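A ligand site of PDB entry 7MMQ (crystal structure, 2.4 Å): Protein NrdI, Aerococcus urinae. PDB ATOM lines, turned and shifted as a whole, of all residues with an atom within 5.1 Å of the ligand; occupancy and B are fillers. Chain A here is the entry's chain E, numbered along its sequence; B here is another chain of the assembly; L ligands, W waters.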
ATOM      1  N   PHE A  13      19.234 -20.171 -24.807  1.00  0.00           N
ATOM      2  CA  PHE A  13      19.637 -20.798 -23.521  1.00  0.00           C
ATOM      3  C   PHE A  13      18.908 -22.138 -23.392  1.00  0.00           C
ATOM      4  O   PHE A  13      17.773 -22.272 -23.886  1.00  0.00           O
ATOM      5  CB  PHE A  13      19.322 -19.900 -22.321  1.00  0.00           C
ATOM      6  CG  PHE A  13      19.641 -20.537 -20.993  1.00  0.00           C
ATOM      7  CD1 PHE A  13      20.945 -20.612 -20.542  1.00  0.00           C
ATOM      8  CD2 PHE A  13      18.649 -21.100 -20.222  1.00  0.00           C
ATOM      9  CE1 PHE A  13      21.246 -21.201 -19.323  1.00  0.00           C
ATOM     10  CE2 PHE A  13      18.940 -21.700 -19.004  1.00  0.00           C
ATOM     11  CZ  PHE A  13      20.241 -21.752 -18.561  1.00  0.00           C
ATOM     12  N   SER A  14      19.578 -23.097 -22.752  1.00  0.00           N
ATOM     13  CA  SER A  14      19.042 -24.447 -22.450  1.00  0.00           C
ATOM     14  C   SER A  14      19.757 -24.983 -21.205  1.00  0.00           C
ATOM     15  O   SER A  14      20.988 -24.815 -21.119  1.00  0.00           O
ATOM     16  CB  SER A  14      19.196 -25.352 -23.647  1.00  0.00           C
ATOM     17  OG  SER A  14      18.300 -26.443 -23.582  1.00  0.00           O
ATOM     18  N   THR A  15      19.014 -25.559 -20.278  1.00  0.00           N
ATOM     19  CA  THR A  15      19.569 -26.169 -19.033  1.00  0.00           C
ATOM     20  C   THR A  15      20.132 -27.556 -19.383  1.00  0.00           C
ATOM     21  O   THR A  15      20.203 -27.879 -20.582  1.00  0.00           O
ATOM     22  CB  THR A  15      18.505 -26.222 -17.928  1.00  0.00           C
ATOM     23  OG1 THR A  15      17.469 -27.118 -18.334  1.00  0.00           O
ATOM     24  CG2 THR A  15      17.917 -24.868 -17.609  1.00  0.00           C
ATOM     25  N   SER A  17      18.858 -30.371 -19.224  1.00  0.00           N
ATOM     26  CA  SER A  17      17.818 -31.226 -19.859  1.00  0.00           C
ATOM     27  C   SER A  17      17.797 -31.071 -21.386  1.00  0.00           C
ATOM     28  O   SER A  17      17.304 -32.001 -22.052  1.00  0.00           O
ATOM     29  CB  SER A  17      16.457 -30.990 -19.244  1.00  0.00           C
ATOM     30  OG  SER A  17      16.111 -29.614 -19.249  1.00  0.00           O
ATOM     31  N   ASN A  18      18.279 -29.949 -21.922  1.00  0.00           N
ATOM     32  CA  ASN A  18      18.630 -29.762 -23.369  1.00  0.00           C
ATOM     33  C   ASN A  18      17.398 -29.801 -24.286  1.00  0.00           C
ATOM     34  O   ASN A  18      17.563 -30.133 -25.477  1.00  0.00           O
ATOM     35  CB  ASN A  18      19.670 -30.784 -23.830  1.00  0.00           C
ATOM     36  CG  ASN A  18      21.078 -30.455 -23.402  1.00  0.00           C
ATOM     37  OD1 ASN A  18      21.522 -29.313 -23.564  1.00  0.00           O
ATOM     38  ND2 ASN A  18      21.798 -31.426 -22.873  1.00  0.00           N
ATOM     39  N   ASN A  19      16.202 -29.441 -23.789  1.00  0.00           N
ATOM     40  CA  ASN A  19      14.961 -29.438 -24.612  1.00  0.00           C
ATOM     41  C   ASN A  19      15.066 -28.326 -25.663  1.00  0.00           C
ATOM     42  O   ASN A  19      14.827 -28.606 -26.862  1.00  0.00           O
ATOM     43  CB  ASN A  19      13.689 -29.251 -23.790  1.00  0.00           C
ATOM     44  CG  ASN A  19      13.304 -30.463 -22.959  1.00  0.00           C
ATOM     45  OD1 ASN A  19      13.814 -31.558 -23.168  1.00  0.00           O
ATOM     46  ND2 ASN A  19      12.388 -30.270 -22.024  1.00  0.00           N
ATOM     47  N   THR A  20      15.423 -27.109 -25.234  1.00  0.00           N
ATOM     48  CA  THR A  20      15.517 -25.908 -26.104  1.00  0.00           C
ATOM     49  C   THR A  20      16.674 -26.108 -27.086  1.00  0.00           C
ATOM     50  O   THR A  20      16.491 -25.809 -28.270  1.00  0.00           O
ATOM     51  CB  THR A  20      15.652 -24.630 -25.267  1.00  0.00           C
ATOM     52  OG1 THR A  20      14.676 -24.683 -24.222  1.00  0.00           O
ATOM     53  CG2 THR A  20      15.462 -23.365 -26.078  1.00  0.00           C
ATOM     54  N   HIS A  21      17.804 -26.619 -26.597  1.00  0.00           N
ATOM     55  CA  HIS A  21      18.994 -26.960 -27.418  1.00  0.00           C
ATOM     56  C   HIS A  21      18.541 -27.811 -28.616  1.00  0.00           C
ATOM     57  O   HIS A  21      18.825 -27.393 -29.759  1.00  0.00           O
ATOM     58  CB  HIS A  21      20.067 -27.672 -26.580  1.00  0.00           C
ATOM     59  CG  HIS A  21      21.189 -28.239 -27.389  1.00  0.00           C
ATOM     60  ND1 HIS A  21      22.155 -27.448 -27.989  1.00  0.00           N
ATOM     61  CD2 HIS A  21      21.502 -29.524 -27.702  1.00  0.00           C
ATOM     62  CE1 HIS A  21      23.014 -28.223 -28.629  1.00  0.00           C
ATOM     63  NE2 HIS A  21      22.637 -29.493 -28.472  1.00  0.00           N
ATOM     64  N   PRO A  53      13.738 -21.067 -22.576  1.00  0.00           N
ATOM     65  CA  PRO A  53      12.693 -21.697 -21.773  1.00  0.00           C
ATOM     66  C   PRO A  53      12.305 -20.838 -20.564  1.00  0.00           C
ATOM     67  O   PRO A  53      12.898 -19.790 -20.355  1.00  0.00           O
ATOM     68  CB  PRO A  53      13.343 -23.012 -21.344  1.00  0.00           C
ATOM     69  CG  PRO A  53      14.817 -22.656 -21.200  1.00  0.00           C
ATOM     70  CD  PRO A  53      15.068 -21.627 -22.287  1.00  0.00           C
ATOM     71  N   THR A  54      11.325 -21.317 -19.784  1.00  0.00           N
ATOM     72  CA  THR A  54      10.704 -20.596 -18.647  1.00  0.00           C
ATOM     73  C   THR A  54      10.851 -21.459 -17.378  1.00  0.00           C
ATOM     74  O   THR A  54      10.671 -22.687 -17.474  1.00  0.00           O
ATOM     75  CB  THR A  54       9.244 -20.261 -18.963  1.00  0.00           C
ATOM     76  OG1 THR A  54       9.210 -19.701 -20.275  1.00  0.00           O
ATOM     77  CG2 THR A  54       8.623 -19.316 -17.968  1.00  0.00           C
ATOM     78  N   TYR A  55      11.181 -20.809 -16.252  1.00  0.00           N
ATOM     79  CA  TYR A  55      11.426 -21.447 -14.929  1.00  0.00           C
ATOM     80  C   TYR A  55      10.975 -20.499 -13.798  1.00  0.00           C
ATOM     81  O   TYR A  55      11.837 -19.794 -13.241  1.00  0.00           O
ATOM     82  CB  TYR A  55      12.912 -21.799 -14.787  1.00  0.00           C
ATOM     83  CG  TYR A  55      13.373 -22.978 -15.621  1.00  0.00           C
ATOM     84  CD1 TYR A  55      13.232 -24.274 -15.151  1.00  0.00           C
ATOM     85  CD2 TYR A  55      13.935 -22.799 -16.874  1.00  0.00           C
ATOM     86  CE1 TYR A  55      13.642 -25.362 -15.899  1.00  0.00           C
ATOM     87  CE2 TYR A  55      14.359 -23.881 -17.634  1.00  0.00           C
ATOM     88  CZ  TYR A  55      14.207 -25.176 -17.145  1.00  0.00           C
ATOM     89  OH  TYR A  55      14.608 -26.247 -17.878  1.00  0.00           O
ATOM     90  N   SER A  56       9.671 -20.493 -13.469  1.00  0.00           N
ATOM     91  CA  SER A  56       9.090 -19.714 -12.334  1.00  0.00           C
ATOM     92  C   SER A  56       8.533 -20.664 -11.273  1.00  0.00           C
ATOM     93  O   SER A  56       8.041 -21.750 -11.661  1.00  0.00           O
ATOM     94  CB  SER A  56       8.038 -18.758 -12.822  1.00  0.00           C
ATOM     95  OG  SER A  56       7.015 -19.444 -13.542  1.00  0.00           O
ATOM     96  N   SER A  95       9.706 -20.964 -24.641  1.00  0.00           N
ATOM     97  CA  SER A  95       9.236 -22.359 -24.497  1.00  0.00           C
ATOM     98  C   SER A  95       8.828 -22.609 -23.052  1.00  0.00           C
ATOM     99  O   SER A  95       9.138 -21.768 -22.175  1.00  0.00           O
ATOM    100  CB  SER A  95      10.259 -23.356 -24.965  1.00  0.00           C
ATOM    101  OG  SER A  95      11.280 -23.528 -23.984  1.00  0.00           O
ATOM    102  N   GLY A  96       8.161 -23.742 -22.821  1.00  0.00           N
ATOM    103  CA  GLY A  96       7.764 -24.217 -21.499  1.00  0.00           C
ATOM    104  C   GLY A  96       6.778 -25.362 -21.602  1.00  0.00           C
ATOM    105  O   GLY A  96       6.965 -26.224 -22.476  1.00  0.00           O
ATOM    106  N   ASN A  97       5.746 -25.357 -20.756  1.00  0.00           N
ATOM    107  CA  ASN A  97       4.711 -26.417 -20.691  1.00  0.00           C
ATOM    108  C   ASN A  97       3.401 -25.759 -20.269  1.00  0.00           C
ATOM    109  O   ASN A  97       3.411 -24.995 -19.279  1.00  0.00           O
ATOM    110  CB  ASN A  97       5.166 -27.554 -19.778  1.00  0.00           C
ATOM    111  CG  ASN A  97       4.464 -28.864 -20.075  1.00  0.00           C
ATOM    112  OD1 ASN A  97       3.236 -28.924 -20.083  1.00  0.00           O
ATOM    113  ND2 ASN A  97       5.226 -29.930 -20.298  1.00  0.00           N
ATOM    114  N   PHE A 100       1.558 -25.355 -16.654  1.00  0.00           N
ATOM    115  CA  PHE A 100       1.902 -24.252 -15.712  1.00  0.00           C
ATOM    116  C   PHE A 100       0.847 -23.138 -15.776  1.00  0.00           C
ATOM    117  O   PHE A 100       0.952 -22.185 -14.983  1.00  0.00           O
ATOM    118  CB  PHE A 100       3.312 -23.734 -16.014  1.00  0.00           C
ATOM    119  CG  PHE A 100       4.399 -24.671 -15.574  1.00  0.00           C
ATOM    120  CD1 PHE A 100       4.904 -24.608 -14.276  1.00  0.00           C
ATOM    121  CD2 PHE A 100       4.894 -25.642 -16.421  1.00  0.00           C
ATOM    122  CE1 PHE A 100       5.897 -25.488 -13.867  1.00  0.00           C
ATOM    123  CE2 PHE A 100       5.874 -26.520 -16.010  1.00  0.00           C
ATOM    124  CZ  PHE A 100       6.370 -26.448 -14.733  1.00  0.00           C
ATOM    125  N   SER A 103       1.500 -19.314 -16.066  1.00  0.00           N
ATOM    126  CA  SER A 103       2.984 -19.256 -16.100  1.00  0.00           C
ATOM    127  C   SER A 103       3.547 -19.850 -17.402  1.00  0.00           C
ATOM    128  O   SER A 103       4.765 -19.802 -17.576  1.00  0.00           O
ATOM    129  CB  SER A 103       3.571 -19.961 -14.900  1.00  0.00           C
ATOM    130  OG  SER A 103       3.419 -19.171 -13.728  1.00  0.00           O
ATOM    131  N   PHE A 104       2.703 -20.376 -18.300  1.00  0.00           N
ATOM    132  CA  PHE A 104       3.169 -21.008 -19.557  1.00  0.00           C
ATOM    133  C   PHE A 104       3.959 -19.982 -20.386  1.00  0.00           C
ATOM    134  O   PHE A 104       3.344 -18.993 -20.864  1.00  0.00           O
ATOM    135  CB  PHE A 104       2.025 -21.579 -20.391  1.00  0.00           C
ATOM    136  CG  PHE A 104       2.427 -21.976 -21.794  1.00  0.00           C
ATOM    137  CD1 PHE A 104       3.525 -22.802 -22.002  1.00  0.00           C
ATOM    138  CD2 PHE A 104       1.735 -21.513 -22.904  1.00  0.00           C
ATOM    139  CE1 PHE A 104       3.913 -23.161 -23.287  1.00  0.00           C
ATOM    140  CE2 PHE A 104       2.116 -21.876 -24.183  1.00  0.00           C
ATOM    141  CZ  PHE A 104       3.201 -22.701 -24.372  1.00  0.00           C
ATOM    142  N   ALA A 105       5.268 -20.219 -20.522  1.00  0.00           N
ATOM    143  CA  ALA A 105       6.191 -19.558 -21.485  1.00  0.00           C
ATOM    144  C   ALA A 105       6.323 -18.046 -21.197  1.00  0.00           C
ATOM    145  O   ALA A 105       6.681 -17.320 -22.139  1.00  0.00           O
ATOM    146  CB  ALA A 105       5.701 -19.802 -22.895  1.00  0.00           C
ATOM    147  N   GLU A 124       6.615 -25.838 -26.883  1.00  0.00           N
ATOM    148  CA  GLU A 124       6.671 -26.811 -25.765  1.00  0.00           C
ATOM    149  C   GLU A 124       7.841 -27.790 -25.952  1.00  0.00           C
ATOM    150  O   GLU A 124       7.991 -28.342 -27.064  1.00  0.00           O
ATOM    151  CB  GLU A 124       5.354 -27.597 -25.675  1.00  0.00           C
ATOM    152  CG  GLU A 124       4.202 -26.783 -25.113  1.00  0.00           C
ATOM    153  CD  GLU A 124       3.018 -27.609 -24.643  1.00  0.00           C
ATOM    154  OE1 GLU A 124       2.261 -28.120 -25.512  1.00  0.00           O
ATOM    155  OE2 GLU A 124       2.852 -27.755 -23.412  1.00  0.00           O
ATOM    156  N   LEU A 125       8.628 -27.984 -24.882  1.00  0.00           N
ATOM    157  CA  LEU A 125       9.708 -29.007 -24.774  1.00  0.00           C
ATOM    158  C   LEU A 125      10.645 -28.903 -25.983  1.00  0.00           C
ATOM    159  O   LEU A 125      11.312 -27.860 -26.114  1.00  0.00           O
ATOM    160  CB  LEU A 125       9.087 -30.407 -24.663  1.00  0.00           C
ATOM    161  CG  LEU A 125       8.316 -30.761 -23.389  1.00  0.00           C
ATOM    162  CD1 LEU A 125       8.511 -29.739 -22.274  1.00  0.00           C
ATOM    163  CD2 LEU A 125       6.838 -30.944 -23.693  1.00  0.00           C
ATOM    164  N   LYS B  41      20.064 -30.011 -11.550  1.00  0.00           N
ATOM    165  CA  LYS B  41      18.654 -30.204 -11.990  1.00  0.00           C
ATOM    166  C   LYS B  41      17.830 -30.809 -10.848  1.00  0.00           C
ATOM    167  O   LYS B  41      16.635 -30.464 -10.733  1.00  0.00           O
ATOM    168  CB  LYS B  41      18.626 -31.074 -13.253  1.00  0.00           C
ATOM    169  CG  LYS B  41      17.245 -31.316 -13.848  1.00  0.00           C
ATOM    170  CD  LYS B  41      16.520 -30.047 -14.275  1.00  0.00           C
ATOM    171  CE  LYS B  41      17.221 -29.312 -15.395  1.00  0.00           C
ATOM    172  NZ  LYS B  41      16.288 -28.371 -16.077  1.00  0.00           N
ATOM    173  N   GLU B  44      16.841 -27.897  -8.589  1.00  0.00           N
ATOM    174  CA  GLU B  44      15.766 -27.142  -9.275  1.00  0.00           C
ATOM    175  C   GLU B  44      14.416 -27.819  -8.987  1.00  0.00           C
ATOM    176  O   GLU B  44      13.481 -27.132  -8.514  1.00  0.00           O
ATOM    177  CB  GLU B  44      15.966 -27.083 -10.789  1.00  0.00           C
ATOM    178  CG  GLU B  44      17.230 -26.349 -11.231  1.00  0.00           C
ATOM    179  CD  GLU B  44      17.474 -26.398 -12.733  1.00  0.00           C
ATOM    180  OE1 GLU B  44      16.496 -26.176 -13.507  1.00  0.00           O
ATOM    181  OE2 GLU B  44      18.636 -26.662 -13.139  1.00  0.00           O
ATOM    182  N   VAL B  45      14.334 -29.129  -9.272  1.00  0.00           N
ATOM    183  CA  VAL B  45      13.099 -29.962  -9.142  1.00  0.00           C
ATOM    184  C   VAL B  45      12.686 -30.046  -7.664  1.00  0.00           C
ATOM    185  O   VAL B  45      11.496 -29.807  -7.388  1.00  0.00           O
ATOM    186  CB  VAL B  45      13.305 -31.356  -9.787  1.00  0.00           C
ATOM    187  CG1 VAL B  45      12.233 -32.338  -9.382  1.00  0.00           C
ATOM    188  CG2 VAL B  45      13.383 -31.253 -11.307  1.00  0.00           C
ATOM    189  N   ARG B  48      11.278 -26.755  -6.335  1.00  0.00           N
ATOM    190  CA  ARG B  48       9.984 -26.433  -7.002  1.00  0.00           C
ATOM    191  C   ARG B  48       8.860 -27.271  -6.370  1.00  0.00           C
ATOM    192  O   ARG B  48       7.859 -26.665  -5.954  1.00  0.00           O
ATOM    193  CB  ARG B  48      10.067 -26.659  -8.511  1.00  0.00           C
ATOM    194  CG  ARG B  48       8.794 -26.322  -9.278  1.00  0.00           C
ATOM    195  CD  ARG B  48       8.258 -24.918  -9.033  1.00  0.00           C
ATOM    196  NE  ARG B  48       9.303 -23.925  -8.844  1.00  0.00           N
ATOM    197  CZ  ARG B  48       9.350 -23.003  -7.874  1.00  0.00           C
ATOM    198  NH1 ARG B  48       8.373 -22.905  -6.980  1.00  0.00           N
ATOM    199  NH2 ARG B  48      10.373 -22.186  -7.804  1.00  0.00           N
ATOM    200  N   ILE B 217       5.906 -31.877 -13.716  1.00  0.00           N
ATOM    201  CA  ILE B 217       7.291 -32.000 -13.179  1.00  0.00           C
ATOM    202  C   ILE B 217       7.626 -33.489 -12.953  1.00  0.00           C
ATOM    203  O   ILE B 217       8.770 -33.877 -13.233  1.00  0.00           O
ATOM    204  CB  ILE B 217       7.489 -31.159 -11.912  1.00  0.00           C
ATOM    205  CG1 ILE B 217       7.354 -29.668 -12.226  1.00  0.00           C
ATOM    206  CG2 ILE B 217       8.826 -31.483 -11.243  1.00  0.00           C
ATOM    207  CD1 ILE B 217       7.536 -28.762 -11.025  1.00  0.00           C
ATOM    208  N   PHE B 220       8.342 -34.812 -16.489  1.00  0.00           N
ATOM    209  CA  PHE B 220       9.639 -34.234 -16.925  1.00  0.00           C
ATOM    210  C   PHE B 220      10.796 -34.996 -16.259  1.00  0.00           C
ATOM    211  O   PHE B 220      11.749 -35.384 -16.977  1.00  0.00           O
ATOM    212  CB  PHE B 220       9.757 -32.748 -16.586  1.00  0.00           C
ATOM    213  CG  PHE B 220      11.194 -32.297 -16.549  1.00  0.00           C
ATOM    214  CD1 PHE B 220      11.908 -32.164 -17.728  1.00  0.00           C
ATOM    215  CD2 PHE B 220      11.861 -32.129 -15.346  1.00  0.00           C
ATOM    216  CE1 PHE B 220      13.251 -31.807 -17.705  1.00  0.00           C
ATOM    217  CE2 PHE B 220      13.190 -31.770 -15.322  1.00  0.00           C
ATOM    218  CZ  PHE B 220      13.887 -31.611 -16.507  1.00  0.00           C
HETATM  219  N1  LIG L   1       7.394 -24.059 -18.207  1.00  0.00           N
HETATM  220  C1  LIG L   1       6.554 -22.986 -18.285  1.00  0.00           C
HETATM  221  O1  LIG L   1       5.932 -22.753 -19.319  1.00  0.00           O
HETATM  222  N2  LIG L   1       6.448 -22.179 -17.180  1.00  0.00           N
HETATM  223  C2  LIG L   1       7.125 -22.382 -15.984  1.00  0.00           C
HETATM  224  O2  LIG L   1       6.950 -21.590 -15.067  1.00  0.00           O
HETATM  225  C3  LIG L   1       7.983 -23.499 -15.924  1.00  0.00           C
HETATM  226  N3  LIG L   1       8.701 -23.784 -14.789  1.00  0.00           N
HETATM  227  C4  LIG L   1       9.433 -24.952 -14.660  1.00  0.00           C
HETATM  228  C5  LIG L   1      10.042 -25.274 -13.461  1.00  0.00           C
HETATM  229  C6  LIG L   1      10.765 -26.425 -13.317  1.00  0.00           C
HETATM  230  C7  LIG L   1      11.420 -26.737 -11.992  1.00  0.00           C
HETATM  231  C8  LIG L   1      10.917 -27.311 -14.442  1.00  0.00           C
HETATM  232  C9  LIG L   1      11.706 -28.578 -14.331  1.00  0.00           C
HETATM  233  C10 LIG L   1      10.317 -26.987 -15.630  1.00  0.00           C
HETATM  234  C11 LIG L   1       9.572 -25.808 -15.768  1.00  0.00           C
HETATM  235  N4  LIG L   1       8.942 -25.464 -16.998  1.00  0.00           N
HETATM  236  C12 LIG L   1       8.114 -24.337 -17.065  1.00  0.00           C
HETATM  237  C13 LIG L   1       9.110 -26.344 -18.182  1.00  0.00           C
HETATM  238  C14 LIG L   1      10.365 -26.039 -18.976  1.00  0.00           C
HETATM  239  O3  LIG L   1      10.388 -24.684 -19.439  1.00  0.00           O
HETATM  240  C15 LIG L   1      10.446 -26.993 -20.155  1.00  0.00           C
HETATM  241  O4  LIG L   1      10.682 -28.307 -19.659  1.00  0.00           O
HETATM  242  C16 LIG L   1      11.532 -26.630 -21.182  1.00  0.00           C
HETATM  243  O5  LIG L   1      11.362 -27.423 -22.359  1.00  0.00           O
HETATM  244  C17 LIG L   1      12.927 -26.848 -20.635  1.00  0.00           C
HETATM  245  O6  LIG L   1      13.899 -26.318 -21.578  1.00  0.00           O
HETATM  246  P1  LIG L   1      15.460 -26.729 -21.427  1.00  0.00           P
HETATM  247  O7  LIG L   1      15.909 -26.157 -20.088  1.00  0.00           O
HETATM  248  O8  LIG L   1      16.136 -26.083 -22.608  1.00  0.00           O
HETATM  249  O9  LIG L   1      15.517 -28.241 -21.476  1.00  0.00           O
HETATM  250  O   HOH W   1      12.238 -26.157 -24.463  1.00  0.00           O
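An oxygen (O8) of the ligand lies within hydrogen-bond range of the side-chain hydroxyl (OG) of Ser 14. The backbone NH (N) of Thr 15 is in hydrogen-bond range of an oxygen (O7) of the ligand, 3.2 Å away. The side-chain hydroxyl (OG1) of Thr 15 sits at hydrogen-bond distance from an oxygen (O7) of the ligand (2.5 Å). OH of Tyr 55 lies within hydrogen-bond range of O7 of the ligand, 2.6 Å away. The backbone NH (N) of Thr 20 sits at hydrogen-bond distance from an oxygen (O8) of the ligand. The side-chain hydroxyl (OG1) of Thr 20 is in hydrogen-bond range of an oxygen (O8) of the ligand (2.6 Å). The backbone NH (N) of Ser 56 lies within hydrogen-bond range of an oxygen (O2) of the ligand (3.3 Å). The side-chain hydroxyl (OG) of Ser 56 is in hydrogen-bond range of an oxygen (O2) of the ligand (2.6 Å). The side-chain hydroxyl of Ser 17 lies within hydrogen-bond range of an oxygen (O9) of the ligand (2.7 Å). An oxygen (O9) of the ligand sits at hydrogen-bond distance from the backbone NH (N) of Asn 19 (2.7 Å). ND2 of Asn 19 sits at hydrogen-bond distance from O5 of the ligand, 3.0 Å away. O of Thr 54 is in hydrogen-bond range of O3 of the ligand, 2.8 Å away. N of Ala 105 sits at hydrogen-bond distance from O1 of the ligand (2.9 Å). O of Ser 103 lies within hydrogen-bond range of N2 of the ligand, 2.9 Å away. N of Asn 97 lies within hydrogen-bond range of O1 of the ligand (3.0 Å). The backbone NH of Asn 18 is in hydrogen-bond range of an oxygen (O9) of the ligand, 3.3 Å away.
The side-chain hydroxyl (OG) of Ser 14 sits at hydrogen-bond distance from the backbone NH (N) of His 21, at 3.1 Å. The side-chain hydroxyl (OH) of Tyr 55 sits at hydrogen-bond distance from the side-chain hydroxyl (OG1) of Thr 15, at 3.0 Å. The side-chain hydroxyl of Thr 15 sits at hydrogen-bond distance from the side-chain hydroxyl of Ser 17. OG1 of Thr 15 sits at hydrogen-bond distance from NZ of Lys 41 of chain B (2.8 Å). The side-chain amino group (NZ) of Lys 41 of chain B is in hydrogen-bond range of the side-chain hydroxyl (OH) of Tyr 55. The side-chain hydroxyl of Ser 17 sits at hydrogen-bond distance from the side-chain amino group of Lys 41 of chain B, 3.4 Å away. OG1 of Thr 54 lies within hydrogen-bond range of O of Ser 95, at 2.8 Å. The backbone carbonyl oxygen (O) of Gly 96 sits at hydrogen-bond distance from the backbone NH (N) of Leu 125, 3.4 Å away.
Residues that only touch the ligand: Pro 53, Gly 96, Phe 100, Phe 104, Leu 125, Arg 48 of chain B and Phe 220 of chain B. The nearest printed residue that does not touch the ligand is Glu 44 of chain B (4.1 Å).
Water W1 lies within hydrogen-bond range of the backbone carbonyl oxygen of Leu 125, an oxygen (O5) of the ligand, the side-chain hydroxyl of Ser 95 and the side-chain hydroxyl of Thr 20.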
